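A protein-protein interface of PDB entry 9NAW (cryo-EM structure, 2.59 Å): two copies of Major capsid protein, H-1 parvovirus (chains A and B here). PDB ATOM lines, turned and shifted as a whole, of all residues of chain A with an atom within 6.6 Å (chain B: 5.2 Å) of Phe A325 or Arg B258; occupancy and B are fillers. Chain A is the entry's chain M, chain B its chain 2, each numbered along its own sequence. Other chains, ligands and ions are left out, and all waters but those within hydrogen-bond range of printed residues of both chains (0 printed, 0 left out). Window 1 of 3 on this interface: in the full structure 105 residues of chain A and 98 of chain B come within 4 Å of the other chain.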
ATOM      1  N   MET A  67     -16.853 -18.866  -1.832  1.00  0.00           N
ATOM      2  CA  MET A  67     -15.863 -17.912  -2.311  1.00  0.00           C
ATOM      3  C   MET A  67     -14.844 -17.549  -1.242  1.00  0.00           C
ATOM      4  O   MET A  67     -13.655 -17.402  -1.537  1.00  0.00           O
ATOM      5  CB  MET A  67     -16.616 -16.662  -2.712  1.00  0.00           C
ATOM      6  CG  MET A  67     -17.646 -16.925  -3.738  1.00  0.00           C
ATOM      7  SD  MET A  67     -18.577 -15.432  -3.888  1.00  0.00           S
ATOM      8  CE  MET A  67     -19.498 -15.521  -2.368  1.00  0.00           C
ATOM      9  N   ASP A  70     -11.499 -19.599  -0.527  1.00  0.00           N
ATOM     10  CA  ASP A  70     -10.508 -19.783  -1.574  1.00  0.00           C
ATOM     11  C   ASP A  70      -9.101 -19.767  -0.993  1.00  0.00           C
ATOM     12  O   ASP A  70      -8.688 -18.798  -0.355  1.00  0.00           O
ATOM     13  CB  ASP A  70     -10.676 -18.680  -2.614  1.00  0.00           C
ATOM     14  CG  ASP A  70      -9.708 -18.796  -3.758  1.00  0.00           C
ATOM     15  OD1 ASP A  70      -9.804 -19.771  -4.516  1.00  0.00           O
ATOM     16  OD2 ASP A  70      -8.863 -17.897  -3.916  1.00  0.00           O
ATOM     17  N   ASP A  71      -8.379 -20.867  -1.191  1.00  0.00           N
ATOM     18  CA  ASP A  71      -6.954 -20.949  -0.924  1.00  0.00           C
ATOM     19  C   ASP A  71      -6.084 -20.847  -2.163  1.00  0.00           C
ATOM     20  O   ASP A  71      -4.860 -20.909  -2.035  1.00  0.00           O
ATOM     21  CB  ASP A  71      -6.624 -22.255  -0.193  1.00  0.00           C
ATOM     22  CG  ASP A  71      -7.101 -22.256   1.228  1.00  0.00           C
ATOM     23  OD1 ASP A  71      -7.367 -21.168   1.767  1.00  0.00           O
ATOM     24  OD2 ASP A  71      -7.229 -23.350   1.806  1.00  0.00           O
ATOM     25  N   THR A  72      -6.718 -20.825  -3.338  1.00  0.00           N
ATOM     26  CA  THR A  72      -5.975 -20.899  -4.625  1.00  0.00           C
ATOM     27  C   THR A  72      -4.845 -19.879  -4.732  1.00  0.00           C
ATOM     28  O   THR A  72      -5.129 -18.671  -4.643  1.00  0.00           O
ATOM     29  CB  THR A  72      -6.935 -20.765  -5.813  1.00  0.00           C
ATOM     30  OG1 THR A  72      -7.954 -21.753  -5.658  1.00  0.00           O
ATOM     31  CG2 THR A  72      -6.248 -20.942  -7.147  1.00  0.00           C
ATOM     32  N   HIS A  73      -3.618 -20.362  -4.941  1.00  0.00           N
ATOM     33  CA  HIS A  73      -2.507 -19.461  -5.179  1.00  0.00           C
ATOM     34  C   HIS A  73      -1.416 -20.284  -5.830  1.00  0.00           C
ATOM     35  O   HIS A  73      -1.601 -21.462  -6.138  1.00  0.00           O
ATOM     36  CB  HIS A  73      -2.001 -18.833  -3.888  1.00  0.00           C
ATOM     37  CG  HIS A  73      -1.431 -19.826  -2.932  1.00  0.00           C
ATOM     38  ND1 HIS A  73      -2.214 -20.698  -2.212  1.00  0.00           N
ATOM     39  CD2 HIS A  73      -0.153 -20.094  -2.584  1.00  0.00           C
ATOM     40  CE1 HIS A  73      -1.443 -21.461  -1.462  1.00  0.00           C
ATOM     41  NE2 HIS A  73      -0.187 -21.112  -1.668  1.00  0.00           N
ATOM     42  N   TYR A 184       5.039 -15.984  -2.813  1.00  0.00           N
ATOM     43  CA  TYR A 184       3.990 -16.043  -3.817  1.00  0.00           C
ATOM     44  C   TYR A 184       4.553 -15.822  -5.205  1.00  0.00           C
ATOM     45  O   TYR A 184       5.508 -15.070  -5.401  1.00  0.00           O
ATOM     46  CB  TYR A 184       2.908 -15.003  -3.554  1.00  0.00           C
ATOM     47  CG  TYR A 184       2.076 -15.258  -2.338  1.00  0.00           C
ATOM     48  CD1 TYR A 184       0.978 -16.087  -2.402  1.00  0.00           C
ATOM     49  CD2 TYR A 184       2.359 -14.643  -1.140  1.00  0.00           C
ATOM     50  CE1 TYR A 184       0.209 -16.317  -1.308  1.00  0.00           C
ATOM     51  CE2 TYR A 184       1.589 -14.863  -0.040  1.00  0.00           C
ATOM     52  CZ  TYR A 184       0.517 -15.701  -0.133  1.00  0.00           C
ATOM     53  OH  TYR A 184      -0.259 -15.931   0.966  1.00  0.00           O
ATOM     54  N   ARG A 189      -6.082 -15.671 -11.366  1.00  0.00           N
ATOM     55  CA  ARG A 189      -7.092 -16.320 -10.542  1.00  0.00           C
ATOM     56  C   ARG A 189      -8.428 -15.640 -10.766  1.00  0.00           C
ATOM     57  O   ARG A 189      -8.542 -14.423 -10.603  1.00  0.00           O
ATOM     58  CB  ARG A 189      -6.690 -16.282  -9.068  1.00  0.00           C
ATOM     59  CG  ARG A 189      -7.763 -16.733  -8.120  1.00  0.00           C
ATOM     60  CD  ARG A 189      -8.264 -18.083  -8.459  1.00  0.00           C
ATOM     61  NE  ARG A 189      -9.261 -18.517  -7.502  1.00  0.00           N
ATOM     62  CZ  ARG A 189     -10.111 -19.498  -7.734  1.00  0.00           C
ATOM     63  NH1 ARG A 189     -10.984 -19.855  -6.816  1.00  0.00           N
ATOM     64  NH2 ARG A 189     -10.096 -20.109  -8.897  1.00  0.00           N
ATOM     65  N   ASN A 316     -16.043  -6.485   3.454  1.00  0.00           N
ATOM     66  CA  ASN A 316     -15.748  -6.156   2.040  1.00  0.00           C
ATOM     67  C   ASN A 316     -14.781  -7.149   1.407  1.00  0.00           C
ATOM     68  O   ASN A 316     -13.682  -7.343   1.953  1.00  0.00           O
ATOM     69  CB  ASN A 316     -15.188  -4.737   1.912  1.00  0.00           C
ATOM     70  CG  ASN A 316     -15.001  -4.285   0.478  1.00  0.00           C
ATOM     71  OD1 ASN A 316     -15.469  -4.935  -0.455  1.00  0.00           O
ATOM     72  ND2 ASN A 316     -14.338  -3.157   0.297  1.00  0.00           N
ATOM     73  N   PHE A 317     -15.197  -7.746   0.303  1.00  0.00           N
ATOM     74  CA  PHE A 317     -14.362  -8.634  -0.492  1.00  0.00           C
ATOM     75  C   PHE A 317     -14.151  -8.017  -1.861  1.00  0.00           C
ATOM     76  O   PHE A 317     -15.097  -7.902  -2.644  1.00  0.00           O
ATOM     77  CB  PHE A 317     -14.990 -10.016  -0.624  1.00  0.00           C
ATOM     78  CG  PHE A 317     -15.038 -10.779   0.652  1.00  0.00           C
ATOM     79  CD1 PHE A 317     -13.969 -11.549   1.043  1.00  0.00           C
ATOM     80  CD2 PHE A 317     -16.137 -10.702   1.477  1.00  0.00           C
ATOM     81  CE1 PHE A 317     -14.010 -12.249   2.217  1.00  0.00           C
ATOM     82  CE2 PHE A 317     -16.177 -11.396   2.653  1.00  0.00           C
ATOM     83  CZ  PHE A 317     -15.114 -12.168   3.023  1.00  0.00           C
ATOM     84  N   GLU A 318     -12.918  -7.632  -2.148  1.00  0.00           N
ATOM     85  CA  GLU A 318     -12.544  -7.075  -3.434  1.00  0.00           C
ATOM     86  C   GLU A 318     -11.731  -8.107  -4.198  1.00  0.00           C
ATOM     87  O   GLU A 318     -11.015  -8.909  -3.599  1.00  0.00           O
ATOM     88  CB  GLU A 318     -11.756  -5.782  -3.251  1.00  0.00           C
ATOM     89  CG  GLU A 318     -12.591  -4.681  -2.633  1.00  0.00           C
ATOM     90  CD  GLU A 318     -11.814  -3.414  -2.350  1.00  0.00           C
ATOM     91  OE1 GLU A 318     -10.577  -3.413  -2.481  1.00  0.00           O
ATOM     92  OE2 GLU A 318     -12.440  -2.414  -1.968  1.00  0.00           O
ATOM     93  N   ALA A 319     -11.865  -8.104  -5.516  1.00  0.00           N
ATOM     94  CA  ALA A 319     -11.220  -9.091  -6.363  1.00  0.00           C
ATOM     95  C   ALA A 319     -10.260  -8.429  -7.334  1.00  0.00           C
ATOM     96  O   ALA A 319     -10.492  -7.308  -7.792  1.00  0.00           O
ATOM     97  CB  ALA A 319     -12.250  -9.906  -7.133  1.00  0.00           C
ATOM     98  N   ASN A 320      -9.156  -9.113  -7.601  1.00  0.00           N
ATOM     99  CA  ASN A 320      -8.201  -8.609  -8.610  1.00  0.00           C
ATOM    100  C   ASN A 320      -7.805  -9.812  -9.454  1.00  0.00           C
ATOM    101  O   ASN A 320      -8.440 -10.872  -9.303  1.00  0.00           O
ATOM    102  CB  ASN A 320      -6.921  -8.036  -8.001  1.00  0.00           C
ATOM    103  CG  ASN A 320      -7.103  -6.834  -7.097  1.00  0.00           C
ATOM    104  OD1 ASN A 320      -8.215  -6.366  -6.874  1.00  0.00           O
ATOM    105  ND2 ASN A 320      -6.005  -6.322  -6.566  1.00  0.00           N
ATOM    106  N   GLY A 322      -5.723 -11.709  -8.897  1.00  0.00           N
ATOM    107  CA  GLY A 322      -5.309 -12.762  -7.992  1.00  0.00           C
ATOM    108  C   GLY A 322      -6.401 -13.404  -7.162  1.00  0.00           C
ATOM    109  O   GLY A 322      -6.087 -14.220  -6.293  1.00  0.00           O
ATOM    110  N   GLY A 323      -7.664 -13.073  -7.396  1.00  0.00           N
ATOM    111  CA  GLY A 323      -8.749 -13.703  -6.685  1.00  0.00           C
ATOM    112  C   GLY A 323      -9.381 -12.831  -5.622  1.00  0.00           C
ATOM    113  O   GLY A 323      -8.986 -11.687  -5.405  1.00  0.00           O
ATOM    114  N   PRO A 324     -10.401 -13.360  -4.951  1.00  0.00           N
ATOM    115  CA  PRO A 324     -11.091 -12.579  -3.920  1.00  0.00           C
ATOM    116  C   PRO A 324     -10.283 -12.504  -2.638  1.00  0.00           C
ATOM    117  O   PRO A 324      -9.558 -13.431  -2.280  1.00  0.00           O
ATOM    118  CB  PRO A 324     -12.391 -13.356  -3.709  1.00  0.00           C
ATOM    119  CG  PRO A 324     -12.031 -14.747  -4.040  1.00  0.00           C
ATOM    120  CD  PRO A 324     -10.997 -14.692  -5.121  1.00  0.00           C
ATOM    121  N   PHE A 325     -10.413 -11.382  -1.944  1.00  0.00           N
ATOM    122  CA  PHE A 325      -9.781 -11.199  -0.652  1.00  0.00           C
ATOM    123  C   PHE A 325     -10.622 -10.244   0.171  1.00  0.00           C
ATOM    124  O   PHE A 325     -11.236  -9.324  -0.364  1.00  0.00           O
ATOM    125  CB  PHE A 325      -8.355 -10.650  -0.779  1.00  0.00           C
ATOM    126  CG  PHE A 325      -8.273  -9.332  -1.483  1.00  0.00           C
ATOM    127  CD1 PHE A 325      -8.421  -8.154  -0.787  1.00  0.00           C
ATOM    128  CD2 PHE A 325      -8.031  -9.270  -2.836  1.00  0.00           C
ATOM    129  CE1 PHE A 325      -8.359  -6.947  -1.427  1.00  0.00           C
ATOM    130  CE2 PHE A 325      -7.959  -8.060  -3.480  1.00  0.00           C
ATOM    131  CZ  PHE A 325      -8.121  -6.899  -2.773  1.00  0.00           C
ATOM    132  N   LYS A 326     -10.629 -10.453   1.479  1.00  0.00           N
ATOM    133  CA  LYS A 326     -11.287  -9.518   2.373  1.00  0.00           C
ATOM    134  C   LYS A 326     -10.413  -8.295   2.585  1.00  0.00           C
ATOM    135  O   LYS A 326      -9.213  -8.413   2.835  1.00  0.00           O
ATOM    136  CB  LYS A 326     -11.598 -10.161   3.715  1.00  0.00           C
ATOM    137  CG  LYS A 326     -12.294  -9.200   4.638  1.00  0.00           C
ATOM    138  CD  LYS A 326     -12.744  -9.846   5.905  1.00  0.00           C
ATOM    139  CE  LYS A 326     -13.324  -8.808   6.820  1.00  0.00           C
ATOM    140  NZ  LYS A 326     -12.252  -7.924   7.339  1.00  0.00           N
ATOM    141  N   VAL A 327     -11.016  -7.123   2.486  1.00  0.00           N
ATOM    142  CA  VAL A 327     -10.259  -5.890   2.691  1.00  0.00           C
ATOM    143  C   VAL A 327      -9.948  -5.739   4.172  1.00  0.00           C
ATOM    144  O   VAL A 327     -10.853  -5.864   5.007  1.00  0.00           O
ATOM    145  CB  VAL A 327     -11.045  -4.698   2.168  1.00  0.00           C
ATOM    146  CG1 VAL A 327     -10.320  -3.407   2.468  1.00  0.00           C
ATOM    147  CG2 VAL A 327     -11.250  -4.849   0.699  1.00  0.00           C
ATOM    148  N   PRO A 328      -8.702  -5.482   4.547  1.00  0.00           N
ATOM    149  CA  PRO A 328      -8.388  -5.331   5.965  1.00  0.00           C
ATOM    150  C   PRO A 328      -9.056  -4.101   6.548  1.00  0.00           C
ATOM    151  O   PRO A 328      -9.470  -3.193   5.833  1.00  0.00           O
ATOM    152  CB  PRO A 328      -6.862  -5.220   5.979  1.00  0.00           C
ATOM    153  CG  PRO A 328      -6.521  -4.710   4.641  1.00  0.00           C
ATOM    154  CD  PRO A 328      -7.509  -5.322   3.704  1.00  0.00           C
ATOM    155  N   THR B 256      -1.068  -8.401  -5.491  1.00  0.00           N
ATOM    156  CA  THR B 256      -2.349  -8.019  -4.935  1.00  0.00           C
ATOM    157  C   THR B 256      -2.340  -8.321  -3.442  1.00  0.00           C
ATOM    158  O   THR B 256      -1.310  -8.677  -2.870  1.00  0.00           O
ATOM    159  CB  THR B 256      -3.469  -8.753  -5.654  1.00  0.00           C
ATOM    160  OG1 THR B 256      -3.322 -10.156  -5.441  1.00  0.00           O
ATOM    161  CG2 THR B 256      -3.376  -8.491  -7.136  1.00  0.00           C
ATOM    162  N   ASN B 257      -3.490  -8.170  -2.788  1.00  0.00           N
ATOM    163  CA  ASN B 257      -3.569  -8.557  -1.385  1.00  0.00           C
ATOM    164  C   ASN B 257      -3.460 -10.060  -1.204  1.00  0.00           C
ATOM    165  O   ASN B 257      -3.102 -10.524  -0.122  1.00  0.00           O
ATOM    166  CB  ASN B 257      -4.846  -8.024  -0.749  1.00  0.00           C
ATOM    167  CG  ASN B 257      -4.791  -6.537  -0.509  1.00  0.00           C
ATOM    168  OD1 ASN B 257      -5.677  -5.792  -0.892  1.00  0.00           O
ATOM    169  ND2 ASN B 257      -3.749  -6.102   0.169  1.00  0.00           N
ATOM    170  N   ARG B 258      -3.732 -10.836  -2.246  1.00  0.00           N
ATOM    171  CA  ARG B 258      -3.567 -12.278  -2.136  1.00  0.00           C
ATOM    172  C   ARG B 258      -2.102 -12.678  -2.152  1.00  0.00           C
ATOM    173  O   ARG B 258      -1.761 -13.794  -1.761  1.00  0.00           O
ATOM    174  CB  ARG B 258      -4.324 -12.968  -3.265  1.00  0.00           C
ATOM    175  CG  ARG B 258      -5.810 -12.778  -3.184  1.00  0.00           C
ATOM    176  CD  ARG B 258      -6.347 -13.470  -1.959  1.00  0.00           C
ATOM    177  NE  ARG B 258      -6.143 -14.909  -2.032  1.00  0.00           N
ATOM    178  CZ  ARG B 258      -6.966 -15.752  -2.641  1.00  0.00           C
ATOM    179  NH1 ARG B 258      -8.070 -15.306  -3.208  1.00  0.00           N
ATOM    180  NH2 ARG B 258      -6.693 -17.042  -2.665  1.00  0.00           N
ATOM    181  N   HIS B 259      -1.234 -11.805  -2.642  1.00  0.00           N
ATOM    182  CA  HIS B 259       0.168 -12.118  -2.850  1.00  0.00           C
ATOM    183  C   HIS B 259       1.078 -11.608  -1.738  1.00  0.00           C
ATOM    184  O   HIS B 259       2.300 -11.694  -1.870  1.00  0.00           O
ATOM    185  CB  HIS B 259       0.602 -11.586  -4.205  1.00  0.00           C
ATOM    186  CG  HIS B 259      -0.169 -12.182  -5.336  1.00  0.00           C
ATOM    187  ND1 HIS B 259      -1.361 -11.657  -5.776  1.00  0.00           N
ATOM    188  CD2 HIS B 259       0.034 -13.305  -6.059  1.00  0.00           C
ATOM    189  CE1 HIS B 259      -1.835 -12.401  -6.756  1.00  0.00           C
ATOM    190  NE2 HIS B 259      -1.009 -13.410  -6.946  1.00  0.00           N
ATOM    191  N   LEU B 260       0.530 -11.031  -0.679  1.00  0.00           N
ATOM    192  CA  LEU B 260       1.341 -10.375   0.336  1.00  0.00           C
ATOM    193  C   LEU B 260       1.726 -11.339   1.445  1.00  0.00           C
ATOM    194  O   LEU B 260       0.862 -12.002   2.024  1.00  0.00           O
ATOM    195  CB  LEU B 260       0.606  -9.187   0.941  1.00  0.00           C
ATOM    196  CG  LEU B 260       0.303  -8.032   0.006  1.00  0.00           C
ATOM    197  CD1 LEU B 260      -0.500  -6.997   0.761  1.00  0.00           C
ATOM    198  CD2 LEU B 260       1.583  -7.460  -0.541  1.00  0.00           C
ATOM    199  N   GLU B 299      -6.939 -18.427   2.563  1.00  0.00           N
ATOM    200  CA  GLU B 299      -6.080 -17.435   1.869  1.00  0.00           C
ATOM    201  C   GLU B 299      -6.879 -16.155   1.618  1.00  0.00           C
ATOM    202  O   GLU B 299      -6.272 -15.069   1.621  1.00  0.00           O
ATOM    203  CB  GLU B 299      -5.546 -18.059   0.578  1.00  0.00           C
ATOM    204  CG  GLU B 299      -4.599 -17.160  -0.187  1.00  0.00           C
ATOM    205  CD  GLU B 299      -3.250 -16.945   0.471  1.00  0.00           C
ATOM    206  OE1 GLU B 299      -2.971 -17.600   1.495  1.00  0.00           O
ATOM    207  OE2 GLU B 299      -2.494 -16.100  -0.033  1.00  0.00           O
ATOM    208  N   ALA B 300      -8.195 -16.281   1.426  1.00  0.00           N
ATOM    209  CA  ALA B 300      -9.017 -15.103   1.184  1.00  0.00           C
ATOM    210  C   ALA B 300      -9.302 -14.341   2.471  1.00  0.00           C
ATOM    211  O   ALA B 300      -9.487 -13.121   2.449  1.00  0.00           O
ATOM    212  CB  ALA B 300     -10.320 -15.509   0.508  1.00  0.00           C
ATOM    213  N   ARG B 304      -4.119  -8.960   6.051  1.00  0.00           N
ATOM    214  CA  ARG B 304      -3.030  -8.492   5.213  1.00  0.00           C
ATOM    215  C   ARG B 304      -2.548  -7.155   5.740  1.00  0.00           C
ATOM    216  O   ARG B 304      -3.270  -6.475   6.473  1.00  0.00           O
ATOM    217  CB  ARG B 304      -3.487  -8.350   3.759  1.00  0.00           C
ATOM    218  CG  ARG B 304      -3.947  -9.641   3.132  1.00  0.00           C
ATOM    219  CD  ARG B 304      -2.831 -10.626   2.919  1.00  0.00           C
ATOM    220  NE  ARG B 304      -3.344 -11.815   2.245  1.00  0.00           N
ATOM    221  CZ  ARG B 304      -2.648 -12.919   2.009  1.00  0.00           C
ATOM    222  NH1 ARG B 304      -1.376 -12.994   2.353  1.00  0.00           N
ATOM    223  NH2 ARG B 304      -3.221 -13.938   1.391  1.00  0.00           N
ATOM    224  N   ILE B 308      -4.323  -3.000  -1.263  1.00  0.00           N
ATOM    225  CA  ILE B 308      -3.695  -2.616  -2.519  1.00  0.00           C
ATOM    226  C   ILE B 308      -4.807  -2.293  -3.505  1.00  0.00           C
ATOM    227  O   ILE B 308      -5.622  -3.153  -3.840  1.00  0.00           O
ATOM    228  CB  ILE B 308      -2.765  -3.713  -3.037  1.00  0.00           C
ATOM    229  CG1 ILE B 308      -1.603  -3.877  -2.065  1.00  0.00           C
ATOM    230  CG2 ILE B 308      -2.244  -3.359  -4.397  1.00  0.00           C
ATOM    231  CD1 ILE B 308      -0.755  -5.056  -2.338  1.00  0.00           C
ATOM    232  N   ARG B 379      -9.505  -3.329  -9.842  1.00  0.00           N
ATOM    233  CA  ARG B 379     -10.673  -3.920  -9.139  1.00  0.00           C
ATOM    234  C   ARG B 379     -11.645  -4.548 -10.150  1.00  0.00           C
ATOM    235  O   ARG B 379     -12.241  -3.787 -10.938  1.00  0.00           O
ATOM    236  CB  ARG B 379     -11.441  -2.861  -8.340  1.00  0.00           C
ATOM    237  CG  ARG B 379     -10.764  -2.364  -7.072  1.00  0.00           C
ATOM    238  CD  ARG B 379     -10.496  -3.506  -6.110  1.00  0.00           C
ATOM    239  NE  ARG B 379      -9.746  -3.045  -4.938  1.00  0.00           N
ATOM    240  CZ  ARG B 379      -8.529  -3.456  -4.623  1.00  0.00           C
ATOM    241  NH1 ARG B 379      -7.706  -3.872  -5.568  1.00  0.00           N
ATOM    242  NH2 ARG B 379      -8.133  -3.433  -3.364  1.00  0.00           N
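No position is printed for both chains.
Of the 26 pairs that touch across the chains among the printed residues, none has its exchanged pair printed and touching as well.
OD1 of Asp A71 sits at hydrogen-bond distance from N of Glu B299.
O of Ala B300 sits at hydrogen-bond distance from N of Lys A326, 3.1 Å away.
N of Ala B300 is in hydrogen-bond range of O of Asp A70.
The side-chain carboxylate (OE1) of Glu A318 lies within salt-bridge range of the guanidinium group (NH2) of Arg B379.
The side-chain hydroxyl (OH) of Tyr A184 lies within hydrogen-bond range of the guanidinium group (NH1) of Arg B304 (3.4 Å).
The backbone carbonyl oxygen (O) of Pro A324 lies within hydrogen-bond range of the guanidinium group (NH1) of Arg B258, at 2.6 Å.
NH2 of Arg B258 is in salt-bridge range of OD2 of Asp A70 (2.6 Å).
The backbone carbonyl oxygen (O) of Asp A70 lies close to the backbone NH (N) of Glu B299, at 3.4 Å.
OD1 of Asn A320 sits at hydrogen-bond distance from NH1 of Arg B379 (2.9 Å).
The side-chain carboxylate (OE2) of Glu B299 lies within hydrogen-bond range of the side-chain hydroxyl (OH) of Tyr A184, 2.5 Å away.
The backbone carbonyl oxygen of Thr A72 sits at hydrogen-bond distance from the guanidinium group of Arg B258 (3.0 Å).
Among the printed residues, merely in contact across the chains: Asp A71 with Arg B258 (3.9 Å), Tyr A184 with Arg B258 (3.2 Å), Tyr A184 with His B259 (3.0 Å), Tyr A184 with Leu B260 (3.6 Å), Ala A319 with Arg B379 (3.7 Å), Asn A320 with Thr B256 (3.5 Å), Gly A322 with Arg B258 (3.4 Å), Gly A322 with His B259 (3.7 Å), Gly A323 with Arg B258 (3.7 Å), Pro A324 with Ala B300 (3.6 Å), Phe A325 with Asn B257 (3.0 Å), Phe A325 with Arg B258 (3.7 Å), Phe A325 with Ala B300 (3.7 Å), Phe A325 with Arg B379 (3.5 Å) and Pro A328 with Arg B304 (3.8 Å).
Printed residues of chain B that touch a printed residue of chain A: Thr B256, Asn B257, Arg B258, His B259, Leu B260, Glu B299, Ala B300, Arg B304 and Arg B379.
Hydrophobic or aromatic side chains of chain B within 4 Å of the printed part of chain A: His B259 and Ala B300.
Printed residues of chain A that touch a printed residue of chain B: Asp A70, Asp A71, Thr A72, Tyr A184, Glu A318, Ala A319, Asn A320, Gly A322, Gly A323, Pro A324, Phe A325, Lys A326 and Pro A328.
Among the printed residues, 26 pairs touch across the chains.
Of the printed residues of chain B, Phe A325 touches Asn B257, Arg B258, Ala B300 and Arg B379.
Of the printed residues of chain A, Leu B260 touches Tyr A184 (3.6 Å).
Of the printed residues of chain A, Asn B257 touches Phe A325.
Of the printed residues of chain B, Lys A326 touches Ala B300 (3.1 Å).
Of the printed residues of chain B, Glu A318 touches Arg B379 (2.6 Å).
Of the printed residues of chain B, Tyr A184 touches Arg B258, His B259, Leu B260, Glu B299 and Arg B304.
Ile B308 touches none of the printed residues of chain A.
The nearest residue of chain B that does not touch Phe A325 is Ile B308 (4.6 Å).
The nearest printed residue of chain A that does not touch Arg B304 is Lys A326 (5.4 Å).
The guanidinium group (NH2) of Arg B304 sits at hydrogen-bond distance from the backbone carbonyl oxygen (O) of Arg B258 (3.5 Å).
OG1 of Thr B256 is in hydrogen-bond range of ND1 of His B259 (2.5 Å).
NE of Arg B304 is in hydrogen-bond range of O of Asn B257.
The guanidinium group (NH1) of Arg B304 lies within hydrogen-bond range of the backbone carbonyl oxygen (O) of Leu B260 (2.5 Å).
The backbone carbonyl oxygen (O) of Phe A325 sits at hydrogen-bond distance from the backbone NH (N) of Glu A318 (3.0 Å).
OD1 of Asp A70 sits at hydrogen-bond distance from OG1 of Thr A72, 2.9 Å away.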
